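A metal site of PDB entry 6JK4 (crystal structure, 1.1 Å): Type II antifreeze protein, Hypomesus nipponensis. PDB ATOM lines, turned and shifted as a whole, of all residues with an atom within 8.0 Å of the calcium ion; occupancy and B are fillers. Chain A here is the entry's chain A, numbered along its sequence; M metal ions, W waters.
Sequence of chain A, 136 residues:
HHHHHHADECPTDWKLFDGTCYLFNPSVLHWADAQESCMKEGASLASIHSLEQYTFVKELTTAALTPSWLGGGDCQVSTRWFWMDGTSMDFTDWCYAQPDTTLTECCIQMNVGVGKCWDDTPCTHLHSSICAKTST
The backbone NH (N) of Thr 101 sits at hydrogen-bond distance from the side-chain carboxylate (OD2) of Asp 120 (2.8 Å).
The backbone carbonyl oxygen (O) of Glu 105 is in hydrogen-bond range of the backbone NH (N) of Thr 121, at 3.4 Å.
The backbone carbonyl oxygen of Asp 119 lies within hydrogen-bond range of the side-chain hydroxyl of Thr 121.
N of Asp 119 lies within hydrogen-bond range of O of Gln 109 (2.9 Å).
Of the 19 residues printed, 5 come within 4 Å of the calcium ion.
Along chain A the residues within 4 Å of the calcium ion span positions 98 to 120.
The calcium ion is bound by the backbone carbonyl oxygen (O) of Asp 120, at 2.3 Å.
The calcium ion is bound by the side-chain carboxylate (OD2) of Asp 100 (2.3 Å).
OE1 of Glu 105 binds the calcium ion, at 2.4 Å.
OE1 of Gln 98 binds the calcium ion (2.4 Å).
Water W1 binds the calcium ion, 2.4 Å away.
The side-chain carboxylate (OD1) of Asp 120 is bound to the calcium ion (2.4 Å).
The calcium ion is bound by the side-chain carboxylate (OD1) of Asp 119, at 2.5 Å.
Water W1 bridges OD2 of Asp 119 (2.9 Å) and NE2 of Gln 98 (3.1 Å).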
ATOM      1  N   TRP A  81      -0.625  16.577  10.401  1.00  0.00           N
ATOM      2  CA  TRP A  81      -1.777  17.268   9.768  1.00  0.00           C
ATOM      3  C   TRP A  81      -2.523  16.313   8.847  1.00  0.00           C
ATOM      4  O   TRP A  81      -1.892  15.593   8.066  1.00  0.00           O
ATOM      5  CB  TRP A  81      -1.244  18.467   8.964  1.00  0.00           C
ATOM      6  CG  TRP A  81      -0.481  19.433   9.832  1.00  0.00           C
ATOM      7  CD1 TRP A  81       0.880  19.479  10.040  1.00  0.00           C
ATOM      8  CD2 TRP A  81      -1.034  20.435  10.691  1.00  0.00           C
ATOM      9  NE1 TRP A  81       1.201  20.437  10.990  1.00  0.00           N
ATOM     10  CE2 TRP A  81       0.034  21.050  11.399  1.00  0.00           C
ATOM     11  CE3 TRP A  81      -2.334  20.871  10.948  1.00  0.00           C
ATOM     12  CZ2 TRP A  81      -0.192  22.044  12.348  1.00  0.00           C
ATOM     13  CZ3 TRP A  81      -2.562  21.872  11.873  1.00  0.00           C
ATOM     14  CH2 TRP A  81      -1.484  22.463  12.553  1.00  0.00           C
ATOM     15  N   TRP A  94       0.780  28.938   5.945  1.00  0.00           N
ATOM     16  CA  TRP A  94       0.822  29.423   7.339  1.00  0.00           C
ATOM     17  C   TRP A  94       1.120  30.916   7.420  1.00  0.00           C
ATOM     18  O   TRP A  94       2.090  31.413   6.779  1.00  0.00           O
ATOM     19  CB  TRP A  94       1.867  28.627   8.130  1.00  0.00           C
ATOM     20  CG  TRP A  94       1.515  27.179   8.259  1.00  0.00           C
ATOM     21  CD1 TRP A  94       2.281  26.139   7.832  1.00  0.00           C
ATOM     22  CD2 TRP A  94       0.335  26.604   8.880  1.00  0.00           C
ATOM     23  NE1 TRP A  94       1.660  24.936   8.124  1.00  0.00           N
ATOM     24  CE2 TRP A  94       0.445  25.184   8.728  1.00  0.00           C
ATOM     25  CE3 TRP A  94      -0.804  27.135   9.507  1.00  0.00           C
ATOM     26  CZ2 TRP A  94      -0.522  24.313   9.253  1.00  0.00           C
ATOM     27  CZ3 TRP A  94      -1.772  26.265   9.977  1.00  0.00           C
ATOM     28  CH2 TRP A  94      -1.613  24.869   9.878  1.00  0.00           C
ATOM     29  N   ALA A  97       4.382  33.206  12.288  1.00  0.00           N
ATOM     30  CA  ALA A  97       4.298  32.681  13.636  1.00  0.00           C
ATOM     31  C   ALA A  97       3.381  31.456  13.773  1.00  0.00           C
ATOM     32  O   ALA A  97       3.297  30.920  14.873  1.00  0.00           O
ATOM     33  CB  ALA A  97       4.010  33.721  14.699  1.00  0.00           C
ATOM     34  N   GLN A  98       2.921  30.908  12.648  1.00  0.00           N
ATOM     35  CA  GLN A  98       2.050  29.713  12.629  1.00  0.00           C
ATOM     36  C   GLN A  98       2.858  28.575  11.992  1.00  0.00           C
ATOM     37  O   GLN A  98       3.827  28.816  11.263  1.00  0.00           O
ATOM     38  CB  GLN A  98       0.805  30.012  11.806  1.00  0.00           C
ATOM     39  CG  GLN A  98      -0.052  31.147  12.382  1.00  0.00           C
ATOM     40  CD  GLN A  98      -0.467  30.807  13.801  1.00  0.00           C
ATOM     41  OE1 GLN A  98      -1.089  29.777  14.045  1.00  0.00           O
ATOM     42  NE2 GLN A  98      -0.052  31.623  14.770  1.00  0.00           N
ATOM     43  N   PRO A  99       2.421  27.308  12.162  1.00  0.00           N
ATOM     44  CA  PRO A  99       1.396  26.900  13.130  1.00  0.00           C
ATOM     45  C   PRO A  99       2.005  26.745  14.537  1.00  0.00           C
ATOM     46  O   PRO A  99       3.167  26.427  14.689  1.00  0.00           O
ATOM     47  CB  PRO A  99       0.982  25.495  12.615  1.00  0.00           C
ATOM     48  CG  PRO A  99       2.265  24.959  11.990  1.00  0.00           C
ATOM     49  CD  PRO A  99       3.004  26.165  11.441  1.00  0.00           C
ATOM     50  N   ASP A 100       1.169  26.942  15.538  1.00  0.00           N
ATOM     51  CA  ASP A 100       1.592  26.720  16.915  1.00  0.00           C
ATOM     52  C   ASP A 100       1.864  25.233  17.187  1.00  0.00           C
ATOM     53  O   ASP A 100       2.804  24.889  17.942  1.00  0.00           O
ATOM     54  CB  ASP A 100       0.568  27.258  17.878  1.00  0.00           C
ATOM     55  CG  ASP A 100       0.529  28.774  17.734  1.00  0.00           C
ATOM     56  OD1 ASP A 100       1.389  29.450  18.429  1.00  0.00           O
ATOM     57  OD2 ASP A 100      -0.238  29.316  16.946  1.00  0.00           O
ATOM     58  N   THR A 101       1.021  24.349  16.613  1.00  0.00           N
ATOM     59  CA  THR A 101       1.089  22.871  16.756  1.00  0.00           C
ATOM     60  C   THR A 101       0.563  22.379  18.096  1.00  0.00           C
ATOM     61  O   THR A 101       0.508  21.151  18.335  1.00  0.00           O
ATOM     62  CB  THR A 101       2.452  22.240  16.503  1.00  0.00           C
ATOM     63  OG1 THR A 101       3.331  22.322  17.638  1.00  0.00           O
ATOM     64  CG2 THR A 101       3.141  22.776  15.253  1.00  0.00           C
ATOM     65  N   THR A 102       0.054  23.272  18.924  1.00  0.00           N
ATOM     66  CA  THR A 102      -0.481  22.813  20.222  1.00  0.00           C
ATOM     67  C   THR A 102      -1.884  22.244  20.019  1.00  0.00           C
ATOM     68  O   THR A 102      -2.704  22.770  19.230  1.00  0.00           O
ATOM     69  CB  THR A 102      -0.436  23.938  21.243  1.00  0.00           C
ATOM     70  OG1 THR A 102      -1.082  24.997  20.571  1.00  0.00           O
ATOM     71  CG2 THR A 102       0.993  24.274  21.595  1.00  0.00           C
ATOM     72  N   THR A 104      -4.446  22.538  21.863  1.00  0.00           N
ATOM     73  CA  THR A 104      -5.500  23.498  22.228  1.00  0.00           C
ATOM     74  C   THR A 104      -5.943  24.373  21.041  1.00  0.00           C
ATOM     75  O   THR A 104      -6.992  24.905  21.112  1.00  0.00           O
ATOM     76  CB  THR A 104      -5.053  24.338  23.422  1.00  0.00           C
ATOM     77  OG1 THR A 104      -3.800  24.927  23.104  1.00  0.00           O
ATOM     78  CG2 THR A 104      -4.976  23.493  24.688  1.00  0.00           C
ATOM     79  N   GLU A 105      -5.149  24.458  19.957  1.00  0.00           N
ATOM     80  CA  GLU A 105      -5.575  25.240  18.774  1.00  0.00           C
ATOM     81  C   GLU A 105      -5.197  24.420  17.543  1.00  0.00           C
ATOM     82  O   GLU A 105      -4.258  24.789  16.791  1.00  0.00           O
ATOM     83  CB  GLU A 105      -4.959  26.637  18.813  1.00  0.00           C
ATOM     84  CG  GLU A 105      -3.453  26.688  19.009  1.00  0.00           C
ATOM     85  CD  GLU A 105      -3.024  28.130  19.254  1.00  0.00           C
ATOM     86  OE1 GLU A 105      -2.805  28.853  18.291  1.00  0.00           O
ATOM     87  OE2 GLU A 105      -2.901  28.503  20.431  1.00  0.00           O
ATOM     88  N   CYS A 106      -5.966  23.349  17.296  1.00  0.00           N
ATOM     89  CA  CYS A 106      -5.521  22.359  16.312  1.00  0.00           C
ATOM     90  C   CYS A 106      -6.268  22.353  14.969  1.00  0.00           C
ATOM     91  O   CYS A 106      -5.870  21.609  14.091  1.00  0.00           O
ATOM     92  CB  CYS A 106      -5.487  20.976  16.940  1.00  0.00           C
ATOM     93  SG  CYS A 106      -7.082  20.353  17.539  1.00  0.00           S
ATOM     94  N   CYS A 107      -7.293  23.176  14.823  1.00  0.00           N
ATOM     95  CA  CYS A 107      -8.096  23.237  13.573  1.00  0.00           C
ATOM     96  C   CYS A 107      -7.588  24.345  12.654  1.00  0.00           C
ATOM     97  O   CYS A 107      -7.264  25.451  13.101  1.00  0.00           O
ATOM     98  CB  CYS A 107      -9.575  23.450  13.927  1.00  0.00           C
ATOM     99  SG  CYS A 107     -10.427  22.012  14.578  1.00  0.00           S
ATOM    100  N   GLN A 109      -7.781  27.392  10.296  1.00  0.00           N
ATOM    101  CA  GLN A 109      -8.586  28.549   9.859  1.00  0.00           C
ATOM    102  C   GLN A 109      -7.771  29.268   8.750  1.00  0.00           C
ATOM    103  O   GLN A 109      -6.540  29.447   8.930  1.00  0.00           O
ATOM    104  CB  GLN A 109      -8.730  29.507  11.060  1.00  0.00           C
ATOM    105  CG  GLN A 109      -9.562  30.738  10.793  1.00  0.00           C
ATOM    106  CD  GLN A 109      -9.534  31.809  11.881  1.00  0.00           C
ATOM    107  OE1 GLN A 109     -10.156  32.861  11.721  1.00  0.00           O
ATOM    108  NE2 GLN A 109      -8.812  31.551  12.970  1.00  0.00           N
ATOM    109  N   VAL A 112      -6.792  34.576   7.759  1.00  0.00           N
ATOM    110  CA  VAL A 112      -6.459  35.159   9.053  1.00  0.00           C
ATOM    111  C   VAL A 112      -5.570  36.374   8.818  1.00  0.00           C
ATOM    112  O   VAL A 112      -4.524  36.290   8.155  1.00  0.00           O
ATOM    113  CB  VAL A 112      -5.846  34.133   9.998  1.00  0.00           C
ATOM    114  CG1 VAL A 112      -5.465  34.761  11.339  1.00  0.00           C
ATOM    115  CG2 VAL A 112      -6.807  32.974  10.181  1.00  0.00           C
ATOM    116  N   TRP A 118      -3.104  31.131   6.947  1.00  0.00           N
ATOM    117  CA  TRP A 118      -3.640  30.055   7.809  1.00  0.00           C
ATOM    118  C   TRP A 118      -3.121  30.189   9.243  1.00  0.00           C
ATOM    119  O   TRP A 118      -1.929  30.540   9.476  1.00  0.00           O
ATOM    120  CB  TRP A 118      -3.241  28.678   7.267  1.00  0.00           C
ATOM    121  CG  TRP A 118      -3.747  28.356   5.892  1.00  0.00           C
ATOM    122  CD1 TRP A 118      -4.339  29.169   4.970  1.00  0.00           C
ATOM    123  CD2 TRP A 118      -3.604  27.062   5.280  1.00  0.00           C
ATOM    124  NE1 TRP A 118      -4.590  28.460   3.815  1.00  0.00           N
ATOM    125  CE2 TRP A 118      -4.195  27.156   3.986  1.00  0.00           C
ATOM    126  CE3 TRP A 118      -3.118  25.819   5.711  1.00  0.00           C
ATOM    127  CZ2 TRP A 118      -4.185  26.073   3.100  1.00  0.00           C
ATOM    128  CZ3 TRP A 118      -3.209  24.722   4.849  1.00  0.00           C
ATOM    129  CH2 TRP A 118      -3.712  24.862   3.558  1.00  0.00           C
ATOM    130  N   ASP A 119      -3.969  29.797  10.174  1.00  0.00           N
ATOM    131  CA  ASP A 119      -3.618  29.798  11.606  1.00  0.00           C
ATOM    132  C   ASP A 119      -4.330  28.630  12.277  1.00  0.00           C
ATOM    133  O   ASP A 119      -5.572  28.501  12.094  1.00  0.00           O
ATOM    134  CB  ASP A 119      -4.063  31.129  12.210  1.00  0.00           C
ATOM    135  CG  ASP A 119      -3.781  31.342  13.690  1.00  0.00           C
ATOM    136  OD1 ASP A 119      -3.930  30.401  14.442  1.00  0.00           O
ATOM    137  OD2 ASP A 119      -3.405  32.531  14.071  1.00  0.00           O
ATOM    138  N   ASP A 120      -3.603  27.803  12.988  1.00  0.00           N
ATOM    139  CA  ASP A 120      -4.231  26.694  13.745  1.00  0.00           C
ATOM    140  C   ASP A 120      -4.951  27.311  14.962  1.00  0.00           C
ATOM    141  O   ASP A 120      -4.338  28.052  15.776  1.00  0.00           O
ATOM    142  CB  ASP A 120      -3.218  25.595  14.044  1.00  0.00           C
ATOM    143  CG  ASP A 120      -2.001  25.932  14.867  1.00  0.00           C
ATOM    144  OD1 ASP A 120      -1.652  27.146  15.028  1.00  0.00           O
ATOM    145  OD2 ASP A 120      -1.343  24.955  15.332  1.00  0.00           O
ATOM    146  N   THR A 121      -6.216  27.016  15.118  1.00  0.00           N
ATOM    147  CA  THR A 121      -7.131  27.808  15.916  1.00  0.00           C
ATOM    148  C   THR A 121      -7.902  26.887  16.851  1.00  0.00           C
ATOM    149  O   THR A 121      -8.224  25.753  16.435  1.00  0.00           O
ATOM    150  CB  THR A 121      -8.102  28.519  14.946  1.00  0.00           C
ATOM    151  OG1 THR A 121      -7.370  29.394  14.116  1.00  0.00           O
ATOM    152  CG2 THR A 121      -9.164  29.375  15.636  1.00  0.00           C
ATOM    153  N   PRO A 122      -8.287  27.343  18.054  1.00  0.00           N
ATOM    154  CA  PRO A 122      -9.183  26.520  18.883  1.00  0.00           C
ATOM    155  C   PRO A 122     -10.430  26.138  18.084  1.00  0.00           C
ATOM    156  O   PRO A 122     -11.130  26.956  17.555  1.00  0.00           O
ATOM    157  CB  PRO A 122      -9.526  27.442  20.080  1.00  0.00           C
ATOM    158  CG  PRO A 122      -8.276  28.313  20.183  1.00  0.00           C
ATOM    159  CD  PRO A 122      -7.927  28.600  18.725  1.00  0.00           C
HETATM  160 CA    CA M   1      -2.369  29.236  15.994  1.00  0.00          CA
HETATM  161  O   HOH W   1      -2.458  31.549  16.659  1.00  0.00           O
